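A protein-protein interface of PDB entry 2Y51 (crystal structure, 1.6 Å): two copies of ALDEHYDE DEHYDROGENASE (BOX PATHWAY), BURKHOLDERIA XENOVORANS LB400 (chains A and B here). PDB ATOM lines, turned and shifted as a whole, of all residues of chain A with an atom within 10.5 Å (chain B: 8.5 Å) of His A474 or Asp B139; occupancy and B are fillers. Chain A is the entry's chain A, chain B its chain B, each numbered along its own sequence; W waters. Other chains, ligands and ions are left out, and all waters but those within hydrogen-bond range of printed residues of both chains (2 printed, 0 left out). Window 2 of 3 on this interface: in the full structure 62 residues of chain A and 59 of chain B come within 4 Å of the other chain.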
ATOM      1  N   LEU A 282      19.503  -6.763 -26.027  1.00  0.00           N
ATOM      2  CA  LEU A 282      18.922  -5.432 -25.738  1.00  0.00           C
ATOM      3  C   LEU A 282      19.643  -4.675 -24.624  1.00  0.00           C
ATOM      4  O   LEU A 282      19.844  -3.473 -24.704  1.00  0.00           O
ATOM      5  CB  LEU A 282      17.428  -5.594 -25.465  1.00  0.00           C
ATOM      6  CG  LEU A 282      16.593  -6.301 -26.540  1.00  0.00           C
ATOM      7  CD1 LEU A 282      15.226  -6.422 -25.973  1.00  0.00           C
ATOM      8  CD2 LEU A 282      16.548  -5.631 -27.896  1.00  0.00           C
ATOM      9  N   LYS A 285      23.185  -3.513 -25.892  1.00  0.00           N
ATOM     10  CA  LYS A 285      22.976  -2.381 -26.794  1.00  0.00           C
ATOM     11  C   LYS A 285      22.679  -1.083 -25.987  1.00  0.00           C
ATOM     12  O   LYS A 285      23.159   0.005 -26.336  1.00  0.00           O
ATOM     13  CB  LYS A 285      21.850  -2.676 -27.776  1.00  0.00           C
ATOM     14  CG  LYS A 285      22.355  -3.623 -28.938  1.00  0.00           C
ATOM     15  CD  LYS A 285      21.195  -3.781 -29.931  1.00  0.00           C
ATOM     16  CE  LYS A 285      21.681  -4.406 -31.212  1.00  0.00           C
ATOM     17  NZ  LYS A 285      20.555  -4.852 -32.042  1.00  0.00           N
ATOM     18  N   GLU A 286      21.834  -1.195 -24.976  1.00  0.00           N
ATOM     19  CA  GLU A 286      21.346  -0.001 -24.254  1.00  0.00           C
ATOM     20  C   GLU A 286      22.475   0.595 -23.463  1.00  0.00           C
ATOM     21  O   GLU A 286      22.591   1.793 -23.439  1.00  0.00           O
ATOM     22  CB  GLU A 286      20.149  -0.259 -23.352  1.00  0.00           C
ATOM     23  CG  GLU A 286      19.257   0.967 -23.007  1.00  0.00           C
ATOM     24  CD  GLU A 286      18.480   1.489 -24.263  1.00  0.00           C
ATOM     25  OE1 GLU A 286      18.495   0.834 -25.316  1.00  0.00           O
ATOM     26  OE2 GLU A 286      17.873   2.588 -24.261  1.00  0.00           O
ATOM     27  N   ARG A 289      24.803   2.443 -25.858  1.00  0.00           N
ATOM     28  CA  ARG A 289      24.170   3.693 -26.352  1.00  0.00           C
ATOM     29  C   ARG A 289      24.263   4.784 -25.273  1.00  0.00           C
ATOM     30  O   ARG A 289      24.543   5.938 -25.581  1.00  0.00           O
ATOM     31  CB  ARG A 289      22.701   3.408 -26.741  1.00  0.00           C
ATOM     32  CG  ARG A 289      22.048   4.575 -27.405  1.00  0.00           C
ATOM     33  CD  ARG A 289      20.925   4.010 -28.252  1.00  0.00           C
ATOM     34  NE  ARG A 289      19.689   4.749 -28.048  1.00  0.00           N
ATOM     35  CZ  ARG A 289      18.476   4.199 -27.886  1.00  0.00           C
ATOM     36  NH1 ARG A 289      18.280   2.853 -27.856  1.00  0.00           N
ATOM     37  NH2 ARG A 289      17.452   5.030 -27.716  1.00  0.00           N
ATOM     38  N   ASP A 448       7.597  -9.785 -19.624  1.00  0.00           N
ATOM     39  CA  ASP A 448       6.984  -8.442 -19.461  1.00  0.00           C
ATOM     40  C   ASP A 448       6.241  -8.283 -18.150  1.00  0.00           C
ATOM     41  O   ASP A 448       6.425  -7.313 -17.391  1.00  0.00           O
ATOM     42  CB  ASP A 448       5.983  -8.246 -20.606  1.00  0.00           C
ATOM     43  CG  ASP A 448       6.673  -7.876 -21.922  1.00  0.00           C
ATOM     44  OD1 ASP A 448       7.902  -7.728 -21.956  1.00  0.00           O
ATOM     45  OD2 ASP A 448       5.973  -7.737 -22.916  1.00  0.00           O
ATOM     46  N   HIS A 466      12.424   2.237 -16.315  1.00  0.00           N
ATOM     47  CA  HIS A 466      12.315   2.148 -17.788  1.00  0.00           C
ATOM     48  C   HIS A 466      12.565   0.686 -18.111  1.00  0.00           C
ATOM     49  O   HIS A 466      13.689   0.190 -17.889  1.00  0.00           O
ATOM     50  CB  HIS A 466      13.375   3.053 -18.510  1.00  0.00           C
ATOM     51  CG  HIS A 466      13.208   3.090 -20.010  1.00  0.00           C
ATOM     52  ND1 HIS A 466      13.801   2.187 -20.889  1.00  0.00           N
ATOM     53  CD2 HIS A 466      12.427   3.884 -20.766  1.00  0.00           C
ATOM     54  CE1 HIS A 466      13.428   2.494 -22.138  1.00  0.00           C
ATOM     55  NE2 HIS A 466      12.607   3.517 -22.077  1.00  0.00           N
ATOM     56  N   ALA A 467      11.538  -0.007 -18.644  1.00  0.00           N
ATOM     57  CA  ALA A 467      11.633  -1.482 -18.759  1.00  0.00           C
ATOM     58  C   ALA A 467      11.721  -1.860 -20.217  1.00  0.00           C
ATOM     59  O   ALA A 467      10.848  -1.410 -21.029  1.00  0.00           O
ATOM     60  CB  ALA A 467      10.411  -2.125 -18.115  1.00  0.00           C
ATOM     61  N   ILE A 468      12.780  -2.621 -20.549  1.00  0.00           N
ATOM     62  CA  ILE A 468      13.084  -2.986 -21.949  1.00  0.00           C
ATOM     63  C   ILE A 468      13.042  -4.505 -22.072  1.00  0.00           C
ATOM     64  O   ILE A 468      13.698  -5.216 -21.303  1.00  0.00           O
ATOM     65  CB  ILE A 468      14.460  -2.426 -22.378  1.00  0.00           C
ATOM     66  CG1 ILE A 468      14.375  -0.891 -22.468  1.00  0.00           C
ATOM     67  CG2 ILE A 468      14.958  -3.070 -23.693  1.00  0.00           C
ATOM     68  CD1 ILE A 468      15.808  -0.220 -22.599  1.00  0.00           C
ATOM     69  N   SER A 469      12.287  -4.962 -23.039  1.00  0.00           N
ATOM     70  CA  SER A 469      12.105  -6.387 -23.334  1.00  0.00           C
ATOM     71  C   SER A 469      11.853  -6.558 -24.868  1.00  0.00           C
ATOM     72  O   SER A 469      11.557  -5.557 -25.588  1.00  0.00           O
ATOM     73  CB  SER A 469      10.900  -6.880 -22.549  1.00  0.00           C
ATOM     74  OG  SER A 469       9.773  -6.037 -22.792  1.00  0.00           O
ATOM     75  N   PRO A 470      11.943  -7.822 -25.352  1.00  0.00           N
ATOM     76  CA  PRO A 470      11.814  -8.148 -26.765  1.00  0.00           C
ATOM     77  C   PRO A 470      10.557  -7.618 -27.407  1.00  0.00           C
ATOM     78  O   PRO A 470      10.633  -7.087 -28.538  1.00  0.00           O
ATOM     79  CB  PRO A 470      11.940  -9.694 -26.783  1.00  0.00           C
ATOM     80  CG  PRO A 470      12.805 -10.046 -25.602  1.00  0.00           C
ATOM     81  CD  PRO A 470      12.349  -9.005 -24.551  1.00  0.00           C
ATOM     82  N   SER A 471       9.409  -7.664 -26.699  1.00  0.00           N
ATOM     83  CA  SER A 471       8.172  -7.121 -27.279  1.00  0.00           C
ATOM     84  C   SER A 471       8.181  -5.623 -27.601  1.00  0.00           C
ATOM     85  O   SER A 471       7.345  -5.139 -28.358  1.00  0.00           O
ATOM     86  CB  SER A 471       6.953  -7.475 -26.384  1.00  0.00           C
ATOM     87  OG  SER A 471       6.883  -6.553 -25.297  1.00  0.00           O
ATOM     88  N   VAL A 472       9.120  -4.862 -27.007  1.00  0.00           N
ATOM     89  CA  VAL A 472       9.248  -3.448 -27.299  1.00  0.00           C
ATOM     90  C   VAL A 472      10.642  -3.087 -27.811  1.00  0.00           C
ATOM     91  O   VAL A 472      10.995  -1.897 -27.776  1.00  0.00           O
ATOM     92  CB  VAL A 472       8.876  -2.534 -26.061  1.00  0.00           C
ATOM     93  CG1 VAL A 472       7.417  -2.796 -25.643  1.00  0.00           C
ATOM     94  CG2 VAL A 472       9.719  -2.863 -24.871  1.00  0.00           C
ATOM     95  N   GLN A 473      11.373  -4.057 -28.407  1.00  0.00           N
ATOM     96  CA  GLN A 473      12.676  -3.731 -29.033  1.00  0.00           C
ATOM     97  C   GLN A 473      12.537  -2.590 -30.057  1.00  0.00           C
ATOM     98  O   GLN A 473      13.455  -1.746 -30.197  1.00  0.00           O
ATOM     99  CB  GLN A 473      13.311  -4.924 -29.755  1.00  0.00           C
ATOM    100  CG  GLN A 473      12.401  -5.448 -30.869  1.00  0.00           C
ATOM    101  CD  GLN A 473      13.017  -6.608 -31.633  1.00  0.00           C
ATOM    102  OE1 GLN A 473      14.073  -7.130 -31.252  1.00  0.00           O
ATOM    103  NE2 GLN A 473      12.325  -7.039 -32.727  1.00  0.00           N
ATOM    104  N   HIS A 474      11.410  -2.547 -30.748  1.00  0.00           N
ATOM    105  CA  HIS A 474      11.174  -1.559 -31.805  1.00  0.00           C
ATOM    106  C   HIS A 474      10.511  -0.272 -31.336  1.00  0.00           C
ATOM    107  O   HIS A 474      10.375   0.680 -32.115  1.00  0.00           O
ATOM    108  CB  HIS A 474      10.245  -2.143 -32.841  1.00  0.00           C
ATOM    109  CG  HIS A 474       8.831  -2.358 -32.321  1.00  0.00           C
ATOM    110  ND1 HIS A 474       8.538  -3.191 -31.245  1.00  0.00           N
ATOM    111  CD2 HIS A 474       7.656  -1.760 -32.665  1.00  0.00           C
ATOM    112  CE1 HIS A 474       7.233  -3.137 -30.999  1.00  0.00           C
ATOM    113  NE2 HIS A 474       6.689  -2.237 -31.813  1.00  0.00           N
ATOM    114  N   SER A 475      10.019  -0.246 -30.103  1.00  0.00           N
ATOM    115  CA  SER A 475       9.178   0.873 -29.676  1.00  0.00           C
ATOM    116  C   SER A 475       9.685   1.557 -28.426  1.00  0.00           C
ATOM    117  O   SER A 475       9.278   2.662 -28.140  1.00  0.00           O
ATOM    118  CB  SER A 475       7.735   0.426 -29.397  1.00  0.00           C
ATOM    119  OG  SER A 475       7.655  -0.642 -28.419  1.00  0.00           O
ATOM    120  N   GLN A 476      10.450   0.847 -27.621  1.00  0.00           N
ATOM    121  CA  GLN A 476      10.936   1.427 -26.367  1.00  0.00           C
ATOM    122  C   GLN A 476      11.727   2.710 -26.716  1.00  0.00           C
ATOM    123  O   GLN A 476      12.471   2.766 -27.669  1.00  0.00           O
ATOM    124  CB  GLN A 476      11.763   0.409 -25.563  1.00  0.00           C
ATOM    125  CG  GLN A 476      13.118  -0.017 -26.169  1.00  0.00           C
ATOM    126  CD  GLN A 476      14.290   0.761 -25.630  1.00  0.00           C
ATOM    127  OE1 GLN A 476      14.139   1.724 -24.853  1.00  0.00           O
ATOM    128  NE2 GLN A 476      15.453   0.395 -26.096  1.00  0.00           N
ATOM    129  N   THR A 477      11.608   3.703 -25.833  1.00  0.00           N
ATOM    130  CA  THR A 477      11.971   5.081 -26.198  1.00  0.00           C
ATOM    131  C   THR A 477      13.393   5.427 -25.696  1.00  0.00           C
ATOM    132  O   THR A 477      13.842   6.538 -25.956  1.00  0.00           O
ATOM    133  CB  THR A 477      10.927   6.107 -25.667  1.00  0.00           C
ATOM    134  OG1 THR A 477      10.639   5.871 -24.301  1.00  0.00           O
ATOM    135  CG2 THR A 477       9.635   6.045 -26.504  1.00  0.00           C
ATOM    136  N   GLY A 478      14.037   4.504 -25.004  1.00  0.00           N
ATOM    137  CA  GLY A 478      15.451   4.691 -24.580  1.00  0.00           C
ATOM    138  C   GLY A 478      15.608   4.989 -23.109  1.00  0.00           C
ATOM    139  O   GLY A 478      14.860   5.801 -22.528  1.00  0.00           O
ATOM    140  N   SER B 135       0.163   6.085 -24.021  1.00  0.00           N
ATOM    141  CA  SER B 135       1.017   5.457 -25.058  1.00  0.00           C
ATOM    142  C   SER B 135       2.270   6.282 -25.340  1.00  0.00           C
ATOM    143  O   SER B 135       2.212   7.528 -25.478  1.00  0.00           O
ATOM    144  CB  SER B 135       0.204   5.397 -26.357  1.00  0.00           C
ATOM    145  OG  SER B 135       0.920   4.703 -27.379  1.00  0.00           O
ATOM    146  N   LEU B 136       3.399   5.604 -25.431  1.00  0.00           N
ATOM    147  CA  LEU B 136       4.617   6.200 -25.903  1.00  0.00           C
ATOM    148  C   LEU B 136       5.051   5.660 -27.303  1.00  0.00           C
ATOM    149  O   LEU B 136       6.221   5.846 -27.722  1.00  0.00           O
ATOM    150  CB  LEU B 136       5.729   5.883 -24.862  1.00  0.00           C
ATOM    151  CG  LEU B 136       5.670   6.599 -23.541  1.00  0.00           C
ATOM    152  CD1 LEU B 136       6.610   5.848 -22.646  1.00  0.00           C
ATOM    153  CD2 LEU B 136       6.133   8.089 -23.773  1.00  0.00           C
ATOM    154  N   SER B 137       4.100   5.050 -28.047  1.00  0.00           N
ATOM    155  CA  SER B 137       4.484   4.446 -29.314  1.00  0.00           C
ATOM    156  C   SER B 137       3.257   4.415 -30.220  1.00  0.00           C
ATOM    157  O   SER B 137       2.144   4.316 -29.724  1.00  0.00           O
ATOM    158  CB  SER B 137       4.980   3.008 -29.080  1.00  0.00           C
ATOM    159  OG  SER B 137       4.016   2.250 -28.353  1.00  0.00           O
ATOM    160  N   LYS B 138       3.474   4.525 -31.526  1.00  0.00           N
ATOM    161  CA  LYS B 138       2.355   4.496 -32.457  1.00  0.00           C
ATOM    162  C   LYS B 138       1.531   3.214 -32.290  1.00  0.00           C
ATOM    163  O   LYS B 138       0.256   3.245 -32.340  1.00  0.00           O
ATOM    164  CB  LYS B 138       2.834   4.639 -33.911  1.00  0.00           C
ATOM    165  CG  LYS B 138       1.631   4.916 -34.840  1.00  0.00           C
ATOM    166  CD  LYS B 138       1.275   6.432 -34.918  1.00  0.00           C
ATOM    167  CE  LYS B 138      -0.234   6.649 -35.123  1.00  0.00           C
ATOM    168  NZ  LYS B 138      -0.753   5.673 -36.125  1.00  0.00           N
ATOM    169  N   ASP B 139       2.205   2.085 -32.090  1.00  0.00           N
ATOM    170  CA  ASP B 139       1.450   0.815 -32.002  1.00  0.00           C
ATOM    171  C   ASP B 139       0.923   0.533 -30.596  1.00  0.00           C
ATOM    172  O   ASP B 139       0.362  -0.537 -30.363  1.00  0.00           O
ATOM    173  CB  ASP B 139       2.221  -0.409 -32.585  1.00  0.00           C
ATOM    174  CG  ASP B 139       3.462  -0.739 -31.811  1.00  0.00           C
ATOM    175  OD1 ASP B 139       3.755   0.011 -30.831  1.00  0.00           O
ATOM    176  OD2 ASP B 139       4.143  -1.720 -32.189  1.00  0.00           O
ATOM    177  N   ARG B 140       1.108   1.464 -29.646  1.00  0.00           N
ATOM    178  CA  ARG B 140       0.708   1.294 -28.241  1.00  0.00           C
ATOM    179  C   ARG B 140       1.324   0.109 -27.538  1.00  0.00           C
ATOM    180  O   ARG B 140       0.839  -0.285 -26.449  1.00  0.00           O
ATOM    181  CB  ARG B 140      -0.829   1.141 -28.115  1.00  0.00           C
ATOM    182  CG  ARG B 140      -1.561   2.240 -28.796  1.00  0.00           C
ATOM    183  CD  ARG B 140      -3.080   2.147 -28.480  1.00  0.00           C
ATOM    184  NE  ARG B 140      -3.303   2.822 -27.214  1.00  0.00           N
ATOM    185  CZ  ARG B 140      -3.451   4.147 -27.085  1.00  0.00           C
ATOM    186  NH1 ARG B 140      -3.469   4.948 -28.159  1.00  0.00           N
ATOM    187  NH2 ARG B 140      -3.627   4.671 -25.878  1.00  0.00           N
ATOM    188  N   SER B 141       2.370  -0.477 -28.118  1.00  0.00           N
ATOM    189  CA  SER B 141       3.084  -1.558 -27.486  1.00  0.00           C
ATOM    190  C   SER B 141       3.925  -1.092 -26.261  1.00  0.00           C
ATOM    191  O   SER B 141       4.231  -1.894 -25.397  1.00  0.00           O
ATOM    192  CB  SER B 141       4.051  -2.254 -28.493  1.00  0.00           C
ATOM    193  OG  SER B 141       5.098  -1.361 -28.923  1.00  0.00           O
ATOM    194  N   PHE B 142       4.378   0.152 -26.282  1.00  0.00           N
ATOM    195  CA  PHE B 142       5.161   0.721 -25.163  1.00  0.00           C
ATOM    196  C   PHE B 142       4.419   1.914 -24.506  1.00  0.00           C
ATOM    197  O   PHE B 142       4.023   2.841 -25.182  1.00  0.00           O
ATOM    198  CB  PHE B 142       6.544   1.199 -25.684  1.00  0.00           C
ATOM    199  CG  PHE B 142       7.594   1.525 -24.576  1.00  0.00           C
ATOM    200  CD1 PHE B 142       8.155   0.509 -23.795  1.00  0.00           C
ATOM    201  CD2 PHE B 142       8.088   2.804 -24.454  1.00  0.00           C
ATOM    202  CE1 PHE B 142       9.121   0.749 -22.784  1.00  0.00           C
ATOM    203  CE2 PHE B 142       9.054   3.063 -23.480  1.00  0.00           C
ATOM    204  CZ  PHE B 142       9.596   2.020 -22.679  1.00  0.00           C
ATOM    205  N   SER B 143       4.209   1.889 -23.199  1.00  0.00           N
ATOM    206  CA  SER B 143       3.337   2.882 -22.502  1.00  0.00           C
ATOM    207  C   SER B 143       3.869   3.320 -21.187  1.00  0.00           C
ATOM    208  O   SER B 143       4.820   2.745 -20.693  1.00  0.00           O
ATOM    209  CB  SER B 143       1.910   2.277 -22.301  1.00  0.00           C
ATOM    210  OG  SER B 143       1.439   2.030 -23.599  1.00  0.00           O
ATOM    211  N   SER B 519       3.289  -2.760 -22.737  1.00  0.00           N
ATOM    212  CA  SER B 519       1.937  -2.731 -22.248  1.00  0.00           C
ATOM    213  C   SER B 519       1.532  -3.791 -21.244  1.00  0.00           C
ATOM    214  O   SER B 519       0.767  -3.482 -20.280  1.00  0.00           O
ATOM    215  CB  SER B 519       1.027  -2.985 -23.449  1.00  0.00           C
ATOM    216  OG  SER B 519       0.713  -1.760 -24.014  1.00  0.00           O
HETATM  217  O   HOH W   1       4.368  -4.900 -25.750  1.00  0.00           O
HETATM  218  O   HOH W   2       7.909   4.494 -29.473  1.00  0.00           O
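NE2 of His A474 lies within hydrogen-bond range of OG of Ser B141. The side-chain hydroxyl of Ser B141 lies within hydrogen-bond range of the side-chain hydroxyl of Ser A475 (2.7 Å). NE2 of His A474 lies within hydrogen-bond range of OD2 of Asp B139, 2.6 Å away.
The side-chain carboxylate (OE1) of Glu A286 sits at hydrogen-bond distance from the side-chain amide nitrogen (NE2) of Gln A476 (3.2 Å). The side-chain carboxylate of Asp B139 lies within hydrogen-bond range of the side-chain hydroxyl of Ser B141 (2.7 Å). N of Ser B519 is in hydrogen-bond range of O of Ser B141. The side-chain hydroxyl (OG) of Ser B137 is in hydrogen-bond range of the backbone NH (N) of Ser B141, at 3.2 Å. OE1 of Gln A476 lies within hydrogen-bond range of N of Gly A478, 2.8 Å away. The backbone carbonyl oxygen of Ser B137 lies within hydrogen-bond range of the side-chain hydroxyl of Ser B135 (2.7 Å).
His A466 touches Phe B142 (NE2 to CZ, 3.4 Å). Ala A467 touches Phe B142 (O to CE1, 3.3 Å). O of Ser B141 touches CG1 of Val A472, 3.3 Å away. Phe B142 touches Val A472 (CD1 to CG1, 3.9 Å). Ser A475 touches Ser B137 (CB to CB, 3.8 Å). Ser A475 touches Phe B142 (OG to CB, 3.5 Å). Gln A476 touches Phe B142 (CA to CD2, 3.7 Å). Thr A477 touches Leu B136. Thr A477 touches Phe B142.
Leu A282 touches none of the printed residues of chain B. His A474 touches just these residues of chain B: Asp B139 and Ser B141. Printed residues of chain B within 4 Å of Ser A475: Ser B137 (3.8 Å), Ser B141 (2.7 Å) and Phe B142 (3.5 Å). Ser B135 touches none of the printed residues of chain A. Of chain A, only Ser A475 comes within 4 Å of Ser B137. Asp B139 touches just one residue of chain A: His A474. Of chain A, only Val A472 (3.3 Å), His A474 (3.4 Å) and Ser A475 (2.7 Å) come within 4 Å of Ser B141. Of the printed residues of chain A, Phe B142 touches His A466, Ala A467, Val A472, Ser A475, Gln A476 and Thr A477. The nearest residue of chain B that does not touch His A474 is Ser B137 (6.2 Å). The nearest residue of chain A that does not touch Asp B139 is Ser A475 (4.3 Å).
Of the 18 printed residues of chain A, 7 touch a printed residue of chain B.
No position is printed for both chains.
Water W2 bridges the backbone carbonyl oxygen of Ser A475 (2.6 Å) and the backbone carbonyl oxygen of Leu B136 (2.8 Å). Water W1 lies within hydrogen-bond range of O of Ser B141 (3.0 Å) and OG of Ser A471 (3.0 Å).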
